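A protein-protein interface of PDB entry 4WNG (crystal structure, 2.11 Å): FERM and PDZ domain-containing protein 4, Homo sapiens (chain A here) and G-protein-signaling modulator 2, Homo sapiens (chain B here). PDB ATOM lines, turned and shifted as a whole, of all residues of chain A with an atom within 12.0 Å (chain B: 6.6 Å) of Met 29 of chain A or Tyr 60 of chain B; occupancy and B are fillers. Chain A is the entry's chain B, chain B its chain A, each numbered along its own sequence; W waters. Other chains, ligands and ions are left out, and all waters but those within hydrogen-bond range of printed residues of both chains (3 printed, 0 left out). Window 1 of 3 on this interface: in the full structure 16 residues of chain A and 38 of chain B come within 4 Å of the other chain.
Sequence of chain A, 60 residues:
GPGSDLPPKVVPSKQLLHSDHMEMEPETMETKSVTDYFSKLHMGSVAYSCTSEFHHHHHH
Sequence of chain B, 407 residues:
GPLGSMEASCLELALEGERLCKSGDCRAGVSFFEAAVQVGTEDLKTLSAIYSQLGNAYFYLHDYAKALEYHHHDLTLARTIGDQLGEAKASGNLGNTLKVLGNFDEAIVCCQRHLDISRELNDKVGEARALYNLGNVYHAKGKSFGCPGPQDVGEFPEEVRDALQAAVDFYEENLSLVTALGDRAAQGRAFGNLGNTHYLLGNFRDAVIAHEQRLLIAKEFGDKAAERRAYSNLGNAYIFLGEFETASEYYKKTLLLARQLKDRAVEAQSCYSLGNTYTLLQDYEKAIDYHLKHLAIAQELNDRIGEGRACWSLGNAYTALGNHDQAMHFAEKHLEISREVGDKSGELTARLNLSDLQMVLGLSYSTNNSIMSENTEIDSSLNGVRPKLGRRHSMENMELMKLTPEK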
ATOM      1  N   GLU A  25     -23.888 -29.742 -29.439  1.00  0.00           N
ATOM      2  CA  GLU A  25     -24.050 -28.495 -30.156  1.00  0.00           C
ATOM      3  C   GLU A  25     -23.467 -27.328 -29.333  1.00  0.00           C
ATOM      4  O   GLU A  25     -23.299 -27.452 -28.142  1.00  0.00           O
ATOM      5  CB  GLU A  25     -25.534 -28.263 -30.469  1.00  0.00           C
ATOM      6  CG  GLU A  25     -26.129 -29.345 -31.375  1.00  0.00           C
ATOM      7  CD  GLU A  25     -25.408 -29.407 -32.711  1.00  0.00           C
ATOM      8  OE1 GLU A  25     -25.170 -28.335 -33.293  1.00  0.00           O
ATOM      9  OE2 GLU A  25     -25.022 -30.511 -33.147  1.00  0.00           O
ATOM     10  N   PRO A  26     -23.146 -26.197 -29.981  1.00  0.00           N
ATOM     11  CA  PRO A  26     -22.628 -25.032 -29.234  1.00  0.00           C
ATOM     12  C   PRO A  26     -23.636 -24.319 -28.335  1.00  0.00           C
ATOM     13  O   PRO A  26     -24.842 -24.345 -28.584  1.00  0.00           O
ATOM     14  CB  PRO A  26     -22.171 -24.072 -30.345  1.00  0.00           C
ATOM     15  CG  PRO A  26     -22.911 -24.505 -31.573  1.00  0.00           C
ATOM     16  CD  PRO A  26     -23.042 -26.003 -31.439  1.00  0.00           C
ATOM     17  N   GLU A  27     -23.131 -23.659 -27.293  1.00  0.00           N
ATOM     18  CA  GLU A  27     -23.965 -22.749 -26.513  1.00  0.00           C
ATOM     19  C   GLU A  27     -24.227 -21.557 -27.403  1.00  0.00           C
ATOM     20  O   GLU A  27     -23.395 -21.217 -28.234  1.00  0.00           O
ATOM     21  CB  GLU A  27     -23.261 -22.260 -25.249  1.00  0.00           C
ATOM     22  CG  GLU A  27     -22.840 -23.341 -24.264  1.00  0.00           C
ATOM     23  CD  GLU A  27     -21.431 -23.870 -24.481  1.00  0.00           C
ATOM     24  OE1 GLU A  27     -20.694 -23.359 -25.362  1.00  0.00           O
ATOM     25  OE2 GLU A  27     -21.065 -24.821 -23.768  1.00  0.00           O
ATOM     26  N   THR A  28     -25.396 -20.952 -27.255  1.00  0.00           N
ATOM     27  CA  THR A  28     -25.620 -19.615 -27.746  1.00  0.00           C
ATOM     28  C   THR A  28     -25.256 -18.670 -26.606  1.00  0.00           C
ATOM     29  O   THR A  28     -25.130 -19.088 -25.445  1.00  0.00           O
ATOM     30  CB  THR A  28     -27.096 -19.370 -28.108  1.00  0.00           C
ATOM     31  OG1 THR A  28     -27.919 -19.636 -26.961  1.00  0.00           O
ATOM     32  CG2 THR A  28     -27.535 -20.261 -29.277  1.00  0.00           C
ATOM     33  N   MET A  29     -25.083 -17.399 -26.934  1.00  0.00           N
ATOM     34  CA  MET A  29     -24.972 -16.379 -25.921  1.00  0.00           C
ATOM     35  C   MET A  29     -25.856 -15.271 -26.420  1.00  0.00           C
ATOM     36  O   MET A  29     -26.103 -15.165 -27.618  1.00  0.00           O
ATOM     37  CB  MET A  29     -23.510 -15.921 -25.750  1.00  0.00           C
ATOM     38  CG  MET A  29     -22.556 -17.009 -25.282  1.00  0.00           C
ATOM     39  SD  MET A  29     -22.829 -17.715 -23.630  1.00  0.00           S
ATOM     40  CE  MET A  29     -21.931 -16.571 -22.565  1.00  0.00           C
ATOM     41  N   GLU A  30     -26.380 -14.477 -25.508  1.00  0.00           N
ATOM     42  CA  GLU A  30     -27.199 -13.332 -25.863  1.00  0.00           C
ATOM     43  C   GLU A  30     -26.298 -12.162 -26.118  1.00  0.00           C
ATOM     44  O   GLU A  30     -25.286 -11.986 -25.420  1.00  0.00           O
ATOM     45  CB  GLU A  30     -28.134 -12.975 -24.727  1.00  0.00           C
ATOM     46  CG  GLU A  30     -29.083 -14.091 -24.363  1.00  0.00           C
ATOM     47  CD  GLU A  30     -30.020 -14.413 -25.503  1.00  0.00           C
ATOM     48  OE1 GLU A  30     -30.125 -15.596 -25.850  1.00  0.00           O
ATOM     49  OE2 GLU A  30     -30.625 -13.475 -26.054  1.00  0.00           O
ATOM     50  N   THR A  31     -26.664 -11.339 -27.092  1.00  0.00           N
ATOM     51  CA  THR A  31     -25.796 -10.281 -27.522  1.00  0.00           C
ATOM     52  C   THR A  31     -26.439  -8.938 -27.281  1.00  0.00           C
ATOM     53  O   THR A  31     -27.659  -8.785 -27.356  1.00  0.00           O
ATOM     54  CB  THR A  31     -25.454 -10.399 -29.014  1.00  0.00           C
ATOM     55  OG1 THR A  31     -26.665 -10.330 -29.767  1.00  0.00           O
ATOM     56  CG2 THR A  31     -24.744 -11.708 -29.306  1.00  0.00           C
ATOM     57  N   LYS A  32     -25.582  -7.968 -26.991  1.00  0.00           N
ATOM     58  CA  LYS A  32     -25.957  -6.563 -26.889  1.00  0.00           C
ATOM     59  C   LYS A  32     -25.018  -5.781 -27.798  1.00  0.00           C
ATOM     60  O   LYS A  32     -23.889  -6.212 -28.056  1.00  0.00           O
ATOM     61  CB  LYS A  32     -25.815  -6.080 -25.441  1.00  0.00           C
ATOM     62  CG  LYS A  32     -26.792  -6.753 -24.487  1.00  0.00           C
ATOM     63  CD  LYS A  32     -26.747  -6.166 -23.085  1.00  0.00           C
ATOM     64  CE  LYS A  32     -27.401  -7.136 -22.107  1.00  0.00           C
ATOM     65  NZ  LYS A  32     -27.523  -6.598 -20.738  1.00  0.00           N
ATOM     66  N   SER A  33     -25.476  -4.642 -28.285  1.00  0.00           N
ATOM     67  CA  SER A  33     -24.622  -3.769 -29.082  1.00  0.00           C
ATOM     68  C   SER A  33     -24.829  -2.339 -28.647  1.00  0.00           C
ATOM     69  O   SER A  33     -25.915  -1.978 -28.186  1.00  0.00           O
ATOM     70  CB  SER A  33     -24.935  -3.930 -30.573  1.00  0.00           C
ATOM     71  OG  SER A  33     -24.231  -2.982 -31.359  1.00  0.00           O
ATOM     72  N   ASP A  36     -27.725  -0.458 -30.426  1.00  0.00           N
ATOM     73  CA  ASP A  36     -29.093  -0.543 -29.895  1.00  0.00           C
ATOM     74  C   ASP A  36     -29.597   0.847 -29.522  1.00  0.00           C
ATOM     75  O   ASP A  36     -28.884   1.618 -28.874  1.00  0.00           O
ATOM     76  CB  ASP A  36     -29.161  -1.417 -28.627  1.00  0.00           C
ATOM     77  CG  ASP A  36     -28.907  -2.889 -28.895  1.00  0.00           C
ATOM     78  OD1 ASP A  36     -28.996  -3.308 -30.070  1.00  0.00           O
ATOM     79  OD2 ASP A  36     -28.619  -3.623 -27.916  1.00  0.00           O
ATOM     80  N   CYS B  26     -11.514 -11.848 -31.984  1.00  0.00           N
ATOM     81  CA  CYS B  26     -11.969 -11.535 -30.634  1.00  0.00           C
ATOM     82  C   CYS B  26     -10.843 -10.943 -29.777  1.00  0.00           C
ATOM     83  O   CYS B  26     -11.092 -10.077 -28.944  1.00  0.00           O
ATOM     84  CB  CYS B  26     -12.611 -12.764 -29.964  1.00  0.00           C
ATOM     85  SG  CYS B  26     -14.375 -12.954 -30.359  1.00  0.00           S
ATOM     86  N   GLY B  55     -17.792 -10.083 -21.972  1.00  0.00           N
ATOM     87  CA  GLY B  55     -18.083 -11.404 -21.409  1.00  0.00           C
ATOM     88  C   GLY B  55     -18.132 -12.478 -22.485  1.00  0.00           C
ATOM     89  O   GLY B  55     -17.555 -13.542 -22.331  1.00  0.00           O
ATOM     90  N   ASN B  56     -18.851 -12.206 -23.569  1.00  0.00           N
ATOM     91  CA  ASN B  56     -18.990 -13.182 -24.653  1.00  0.00           C
ATOM     92  C   ASN B  56     -17.659 -13.382 -25.378  1.00  0.00           C
ATOM     93  O   ASN B  56     -17.286 -14.493 -25.677  1.00  0.00           O
ATOM     94  CB  ASN B  56     -20.064 -12.738 -25.641  1.00  0.00           C
ATOM     95  CG  ASN B  56     -21.457 -12.833 -25.056  1.00  0.00           C
ATOM     96  OD1 ASN B  56     -21.672 -13.496 -24.028  1.00  0.00           O
ATOM     97  ND2 ASN B  56     -22.403 -12.157 -25.683  1.00  0.00           N
ATOM     98  N   ALA B  57     -16.925 -12.298 -25.603  1.00  0.00           N
ATOM     99  CA  ALA B  57     -15.624 -12.408 -26.260  1.00  0.00           C
ATOM    100  C   ALA B  57     -14.721 -13.295 -25.431  1.00  0.00           C
ATOM    101  O   ALA B  57     -14.147 -14.243 -25.947  1.00  0.00           O
ATOM    102  CB  ALA B  57     -15.020 -11.037 -26.464  1.00  0.00           C
ATOM    103  N   TYR B  58     -14.651 -13.065 -24.120  1.00  0.00           N
ATOM    104  CA  TYR B  58     -13.813 -13.930 -23.279  1.00  0.00           C
ATOM    105  C   TYR B  58     -14.298 -15.374 -23.247  1.00  0.00           C
ATOM    106  O   TYR B  58     -13.478 -16.303 -23.206  1.00  0.00           O
ATOM    107  CB  TYR B  58     -13.676 -13.385 -21.856  1.00  0.00           C
ATOM    108  CG  TYR B  58     -12.676 -12.258 -21.738  1.00  0.00           C
ATOM    109  CD1 TYR B  58     -11.312 -12.492 -21.903  1.00  0.00           C
ATOM    110  CD2 TYR B  58     -13.090 -10.965 -21.469  1.00  0.00           C
ATOM    111  CE1 TYR B  58     -10.389 -11.460 -21.791  1.00  0.00           C
ATOM    112  CE2 TYR B  58     -12.182  -9.936 -21.343  1.00  0.00           C
ATOM    113  CZ  TYR B  58     -10.831 -10.183 -21.511  1.00  0.00           C
ATOM    114  OH  TYR B  58      -9.928  -9.144 -21.398  1.00  0.00           O
ATOM    115  N   PHE B  59     -15.622 -15.549 -23.262  1.00  0.00           N
ATOM    116  CA  PHE B  59     -16.248 -16.878 -23.319  1.00  0.00           C
ATOM    117  C   PHE B  59     -15.778 -17.610 -24.566  1.00  0.00           C
ATOM    118  O   PHE B  59     -15.315 -18.734 -24.478  1.00  0.00           O
ATOM    119  CB  PHE B  59     -17.791 -16.766 -23.315  1.00  0.00           C
ATOM    120  CG  PHE B  59     -18.509 -18.094 -23.322  1.00  0.00           C
ATOM    121  CD1 PHE B  59     -18.773 -18.761 -24.526  1.00  0.00           C
ATOM    122  CD2 PHE B  59     -18.932 -18.678 -22.148  1.00  0.00           C
ATOM    123  CE1 PHE B  59     -19.432 -19.981 -24.535  1.00  0.00           C
ATOM    124  CE2 PHE B  59     -19.587 -19.905 -22.153  1.00  0.00           C
ATOM    125  CZ  PHE B  59     -19.835 -20.554 -23.345  1.00  0.00           C
ATOM    126  N   TYR B  60     -15.874 -16.967 -25.720  1.00  0.00           N
ATOM    127  CA  TYR B  60     -15.383 -17.593 -26.959  1.00  0.00           C
ATOM    128  C   TYR B  60     -13.870 -17.863 -26.933  1.00  0.00           C
ATOM    129  O   TYR B  60     -13.439 -18.868 -27.449  1.00  0.00           O
ATOM    130  CB  TYR B  60     -15.861 -16.821 -28.191  1.00  0.00           C
ATOM    131  CG  TYR B  60     -17.384 -16.895 -28.306  1.00  0.00           C
ATOM    132  CD1 TYR B  60     -18.031 -18.136 -28.272  1.00  0.00           C
ATOM    133  CD2 TYR B  60     -18.179 -15.744 -28.400  1.00  0.00           C
ATOM    134  CE1 TYR B  60     -19.409 -18.243 -28.348  1.00  0.00           C
ATOM    135  CE2 TYR B  60     -19.568 -15.841 -28.482  1.00  0.00           C
ATOM    136  CZ  TYR B  60     -20.175 -17.099 -28.456  1.00  0.00           C
ATOM    137  OH  TYR B  60     -21.546 -17.255 -28.532  1.00  0.00           O
ATOM    138  N   LEU B  61     -13.094 -17.042 -26.226  1.00  0.00           N
ATOM    139  CA  LEU B  61     -11.660 -17.304 -26.060  1.00  0.00           C
ATOM    140  C   LEU B  61     -11.357 -18.343 -24.991  1.00  0.00           C
ATOM    141  O   LEU B  61     -10.194 -18.655 -24.731  1.00  0.00           O
ATOM    142  CB  LEU B  61     -10.923 -16.012 -25.737  1.00  0.00           C
ATOM    143  CG  LEU B  61     -10.977 -15.002 -26.887  1.00  0.00           C
ATOM    144  CD1 LEU B  61     -10.589 -13.610 -26.413  1.00  0.00           C
ATOM    145  CD2 LEU B  61     -10.104 -15.454 -28.049  1.00  0.00           C
ATOM    146  N   HIS B  62     -12.405 -18.892 -24.383  1.00  0.00           N
ATOM    147  CA  HIS B  62     -12.268 -19.900 -23.336  1.00  0.00           C
ATOM    148  C   HIS B  62     -11.677 -19.335 -22.031  1.00  0.00           C
ATOM    149  O   HIS B  62     -11.172 -20.075 -21.226  1.00  0.00           O
ATOM    150  CB  HIS B  62     -11.460 -21.106 -23.825  1.00  0.00           C
ATOM    151  CG  HIS B  62     -11.902 -21.622 -25.157  1.00  0.00           C
ATOM    152  ND1 HIS B  62     -13.074 -22.329 -25.331  1.00  0.00           N
ATOM    153  CD2 HIS B  62     -11.334 -21.531 -26.383  1.00  0.00           C
ATOM    154  CE1 HIS B  62     -13.209 -22.650 -26.606  1.00  0.00           C
ATOM    155  NE2 HIS B  62     -12.165 -22.179 -27.265  1.00  0.00           N
ATOM    156  N   ASP B  63     -11.758 -18.033 -21.814  1.00  0.00           N
ATOM    157  CA  ASP B  63     -11.358 -17.480 -20.497  1.00  0.00           C
ATOM    158  C   ASP B  63     -12.658 -17.313 -19.715  1.00  0.00           C
ATOM    159  O   ASP B  63     -13.253 -16.239 -19.693  1.00  0.00           O
ATOM    160  CB  ASP B  63     -10.596 -16.154 -20.654  1.00  0.00           C
ATOM    161  CG  ASP B  63      -9.993 -15.650 -19.328  1.00  0.00           C
ATOM    162  OD1 ASP B  63     -10.403 -16.092 -18.221  1.00  0.00           O
ATOM    163  OD2 ASP B  63      -9.107 -14.788 -19.402  1.00  0.00           O
ATOM    164  N   TYR B  64     -13.125 -18.421 -19.155  1.00  0.00           N
ATOM    165  CA  TYR B  64     -14.470 -18.484 -18.578  1.00  0.00           C
ATOM    166  C   TYR B  64     -14.543 -17.691 -17.298  1.00  0.00           C
ATOM    167  O   TYR B  64     -15.565 -17.071 -17.024  1.00  0.00           O
ATOM    168  CB  TYR B  64     -14.894 -19.928 -18.345  1.00  0.00           C
ATOM    169  CG  TYR B  64     -14.978 -20.684 -19.634  1.00  0.00           C
ATOM    170  CD1 TYR B  64     -15.863 -20.294 -20.607  1.00  0.00           C
ATOM    171  CD2 TYR B  64     -14.137 -21.762 -19.903  1.00  0.00           C
ATOM    172  CE1 TYR B  64     -15.946 -20.951 -21.805  1.00  0.00           C
ATOM    173  CE2 TYR B  64     -14.206 -22.423 -21.116  1.00  0.00           C
ATOM    174  CZ  TYR B  64     -15.122 -22.013 -22.054  1.00  0.00           C
ATOM    175  OH  TYR B  64     -15.240 -22.634 -23.271  1.00  0.00           O
ATOM    176  N   ALA B  67     -15.118 -14.223 -18.283  1.00  0.00           N
ATOM    177  CA  ALA B  67     -16.427 -14.093 -18.862  1.00  0.00           C
ATOM    178  C   ALA B  67     -17.404 -13.913 -17.721  1.00  0.00           C
ATOM    179  O   ALA B  67     -18.259 -13.042 -17.784  1.00  0.00           O
ATOM    180  CB  ALA B  67     -16.775 -15.316 -19.689  1.00  0.00           C
ATOM    181  N   HIS B  71     -19.968 -10.711 -17.283  1.00  0.00           N
ATOM    182  CA  HIS B  71     -21.416 -10.934 -17.223  1.00  0.00           C
ATOM    183  C   HIS B  71     -22.018 -10.560 -15.873  1.00  0.00           C
ATOM    184  O   HIS B  71     -23.157 -10.143 -15.812  1.00  0.00           O
ATOM    185  CB  HIS B  71     -21.764 -12.359 -17.618  1.00  0.00           C
ATOM    186  CG  HIS B  71     -21.541 -12.615 -19.063  1.00  0.00           C
ATOM    187  ND1 HIS B  71     -22.002 -11.760 -20.037  1.00  0.00           N
ATOM    188  CD2 HIS B  71     -20.874 -13.601 -19.707  1.00  0.00           C
ATOM    189  CE1 HIS B  71     -21.632 -12.207 -21.225  1.00  0.00           C
ATOM    190  NE2 HIS B  71     -20.944 -13.324 -21.051  1.00  0.00           N
ATOM    191  N   GLY B  92     -28.796 -15.094 -18.565  1.00  0.00           N
ATOM    192  CA  GLY B  92     -28.601 -16.241 -19.445  1.00  0.00           C
ATOM    193  C   GLY B  92     -27.118 -16.402 -19.706  1.00  0.00           C
ATOM    194  O   GLY B  92     -26.569 -17.494 -19.653  1.00  0.00           O
ATOM    195  N   ASN B  93     -26.446 -15.297 -19.943  1.00  0.00           N
ATOM    196  CA  ASN B  93     -25.003 -15.377 -20.200  1.00  0.00           C
ATOM    197  C   ASN B  93     -24.203 -15.906 -19.012  1.00  0.00           C
ATOM    198  O   ASN B  93     -23.318 -16.777 -19.136  1.00  0.00           O
ATOM    199  CB  ASN B  93     -24.532 -14.012 -20.675  1.00  0.00           C
ATOM    200  CG  ASN B  93     -24.992 -13.744 -22.084  1.00  0.00           C
ATOM    201  OD1 ASN B  93     -25.303 -14.701 -22.808  1.00  0.00           O
ATOM    202  ND2 ASN B  93     -25.088 -12.469 -22.476  1.00  0.00           N
ATOM    203  N   LEU B  94     -24.573 -15.418 -17.842  1.00  0.00           N
ATOM    204  CA  LEU B  94     -23.968 -15.846 -16.612  1.00  0.00           C
ATOM    205  C   LEU B  94     -24.207 -17.332 -16.379  1.00  0.00           C
ATOM    206  O   LEU B  94     -23.280 -18.089 -16.059  1.00  0.00           O
ATOM    207  CB  LEU B  94     -24.541 -14.992 -15.477  1.00  0.00           C
ATOM    208  CG  LEU B  94     -23.802 -14.910 -14.156  1.00  0.00           C
ATOM    209  CD1 LEU B  94     -22.367 -14.457 -14.326  1.00  0.00           C
ATOM    210  CD2 LEU B  94     -24.557 -13.980 -13.215  1.00  0.00           C
ATOM    211  N   ASN B  96     -24.888 -19.678 -18.592  1.00  0.00           N
ATOM    212  CA  ASN B  96     -24.108 -20.462 -19.546  1.00  0.00           C
ATOM    213  C   ASN B  96     -22.643 -20.582 -19.110  1.00  0.00           C
ATOM    214  O   ASN B  96     -22.056 -21.667 -19.172  1.00  0.00           O
ATOM    215  CB  ASN B  96     -24.243 -19.873 -20.959  1.00  0.00           C
ATOM    216  CG  ASN B  96     -25.630 -20.103 -21.569  1.00  0.00           C
ATOM    217  OD1 ASN B  96     -26.488 -20.756 -20.978  1.00  0.00           O
ATOM    218  ND2 ASN B  96     -25.852 -19.548 -22.752  1.00  0.00           N
ATOM    219  N   THR B  97     -22.055 -19.484 -18.642  1.00  0.00           N
ATOM    220  CA  THR B  97     -20.628 -19.497 -18.173  1.00  0.00           C
ATOM    221  C   THR B  97     -20.491 -20.370 -16.926  1.00  0.00           C
ATOM    222  O   THR B  97     -19.581 -21.211 -16.808  1.00  0.00           O
ATOM    223  CB  THR B  97     -20.128 -18.062 -17.911  1.00  0.00           C
ATOM    224  OG1 THR B  97     -20.484 -17.228 -19.014  1.00  0.00           O
ATOM    225  CG2 THR B  97     -18.610 -18.010 -17.727  1.00  0.00           C
ATOM    226  N   ARG B 129     -34.616 -19.207 -26.328  1.00  0.00           N
ATOM    227  CA  ARG B 129     -33.173 -19.327 -26.052  1.00  0.00           C
ATOM    228  C   ARG B 129     -32.945 -19.796 -24.639  1.00  0.00           C
ATOM    229  O   ARG B 129     -32.140 -20.709 -24.381  1.00  0.00           O
ATOM    230  CB  ARG B 129     -32.434 -17.997 -26.247  1.00  0.00           C
ATOM    231  CG  ARG B 129     -32.847 -17.161 -27.443  1.00  0.00           C
ATOM    232  CD  ARG B 129     -31.944 -17.324 -28.626  1.00  0.00           C
ATOM    233  NE  ARG B 129     -30.681 -16.613 -28.470  1.00  0.00           N
ATOM    234  CZ  ARG B 129     -29.642 -16.755 -29.295  1.00  0.00           C
ATOM    235  NH1 ARG B 129     -29.729 -17.576 -30.336  1.00  0.00           N
ATOM    236  NH2 ARG B 129     -28.508 -16.089 -29.080  1.00  0.00           N
ATOM    237  N   ASN B 133     -30.948 -23.059 -23.264  1.00  0.00           N
ATOM    238  CA  ASN B 133     -29.934 -22.927 -22.181  1.00  0.00           C
ATOM    239  C   ASN B 133     -30.233 -23.783 -21.001  1.00  0.00           C
ATOM    240  O   ASN B 133     -29.353 -24.427 -20.460  1.00  0.00           O
ATOM    241  CB  ASN B 133     -29.783 -21.464 -21.717  1.00  0.00           C
ATOM    242  CG  ASN B 133     -29.233 -20.573 -22.797  1.00  0.00           C
ATOM    243  OD1 ASN B 133     -28.597 -21.044 -23.722  1.00  0.00           O
ATOM    244  ND2 ASN B 133     -29.465 -19.272 -22.680  1.00  0.00           N
HETATM  245  O   HOH W   1     -28.386 -17.471 -25.250  1.00  0.00           O
HETATM  246  O   HOH W   2     -23.216  -8.960 -25.949  1.00  0.00           O
HETATM  247  O   HOH W   3     -30.402 -20.532 -27.100  1.00  0.00           O
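The backbone carbonyl oxygen (O) of Arg 129 of chain B sits close to the side-chain amide nitrogen (ND2) of Asn 133 of chain B.
The side-chain hydroxyl of Thr 97 of chain B sits at hydrogen-bond distance from the backbone carbonyl oxygen of Asn 93 of chain B, 2.9 Å away.
The side-chain amide nitrogen (ND2) of Asn 96 of chain B is in hydrogen-bond range of the side-chain amide oxygen (OD1) of Asn 133 of chain B, at 3.3 Å.
The side-chain amide oxygen (OD1) of Asn 56 of chain B is in hydrogen-bond range of a ring nitrogen (NE2) of His 71 of chain B (3.1 Å).
Hydrophobic or aromatic side chains of chain A within 4 Å of the printed part of chain B: Met 29.
Hydrophobic or aromatic side chains of chain B within 4 Å of the printed part of chain A: Phe 59, Tyr 60 and His 71.
Among the printed residues, 15 pairs touch across the chains.
Among the printed residues, Asp or Glu carboxylates within 4 Å of a Lys or Arg side-chain nitrogen of the other chain: Glu 30 of chain A with Arg 129 of chain B (2.9 Å).
Printed residues of chain B within 4 Å of Thr 28 of chain A: Asn 96 (2.8 Å), Arg 129 (3.6 Å) and Asn 133 (3.6 Å).
Met 29 of chain A touches just these residues of chain B: Asn 56, Phe 59, Tyr 60, His 71, Asn 93, Asn 96, Thr 97 and Arg 129.
Of the printed residues of chain B, Glu 30 of chain A touches Asn 56, Asn 93 and Arg 129.
No residue of chain A comes within 4 Å of Gly 55 of chain B.
Of chain A, only Met 29 (3.4 Å) and Glu 30 (2.9 Å) come within 4 Å of Asn 56 of chain B.
No residue of chain A comes within 4 Å of Ala 57 of chain B.
Tyr 58 of chain B touches none of the printed residues of chain A.
Phe 59 of chain B touches just these residues of chain A: Glu 27 and Met 29.
Tyr 60 of chain B touches just one residue of chain A: Met 29 (3.4 Å).
No residue of chain A comes within 4 Å of Leu 61 of chain B.
No residue of chain A comes within 4 Å of His 62 of chain B.
Of chain A, only Met 29 comes within 4 Å of Thr 97 of chain B.
Of the printed residues of chain A, Arg 129 of chain B touches Thr 28, Met 29 and Glu 30.
Printed residues of chain A within 4 Å of Asn 133 of chain B: Thr 28 (3.6 Å).
The nearest residue of chain A that does not touch Tyr 60 of chain B is Glu 27 of chain A (4.4 Å).
The nearest printed residue of chain B that does not touch Glu 30 of chain A is Asn 133 of chain B (4.9 Å).
Among the printed residues, pairs that only touch across the chains: Met 29 of chain A with Tyr 60 of chain B, Met 29 of chain A with Asn 56 of chain B, Met 29 of chain A with Asn 93 of chain B, Glu 27 of chain A with Phe 59 of chain B, Thr 28 of chain A with Asn 133 of chain B, Thr 28 of chain A with Arg 129 of chain B, Met 29 of chain A with Phe 59 of chain B, Met 29 of chain A with His 71 of chain B and Met 29 of chain A with Thr 97 of chain B.
Water W1 lies within hydrogen-bond range of the side-chain carboxylate of Glu 30 of chain A (2.6 Å), the side-chain hydroxyl of Thr 28 of chain A (2.8 Å) and the side-chain amide nitrogen of Asn 133 of chain B (3.3 Å).
Water W3 bridges the side-chain hydroxyl of Thr 28 of chain A and the backbone carbonyl oxygen of Arg 129 of chain B.
Water W2 bridges the backbone NH of Lys 32 of chain A (2.8 Å) and the side-chain amide nitrogen of Asn 56 of chain B (3.3 Å).
The side-chain amide nitrogen of Asn 96 of chain B sits at hydrogen-bond distance from the backbone carbonyl oxygen of Thr 28 of chain A (2.8 Å).
NE of Arg 129 of chain B is in salt-bridge range of OE1 of Glu 30 of chain A.
The side-chain amide nitrogen (ND2) of Asn 56 of chain B sits at hydrogen-bond distance from the backbone carbonyl oxygen (O) of Glu 30 of chain A.
The side-chain amide nitrogen (ND2) of Asn 96 of chain B lies within hydrogen-bond range of the side-chain sulfur (SD) of Met 29 of chain A, at 3.6 Å.
The side-chain amide oxygen (OD1) of Asn 93 of chain B is in hydrogen-bond range of the backbone NH (N) of Glu 30 of chain A.
The guanidinium group (NH2) of Arg 129 of chain B sits at hydrogen-bond distance from the backbone carbonyl oxygen (O) of Met 29 of chain A, at 3.0 Å.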
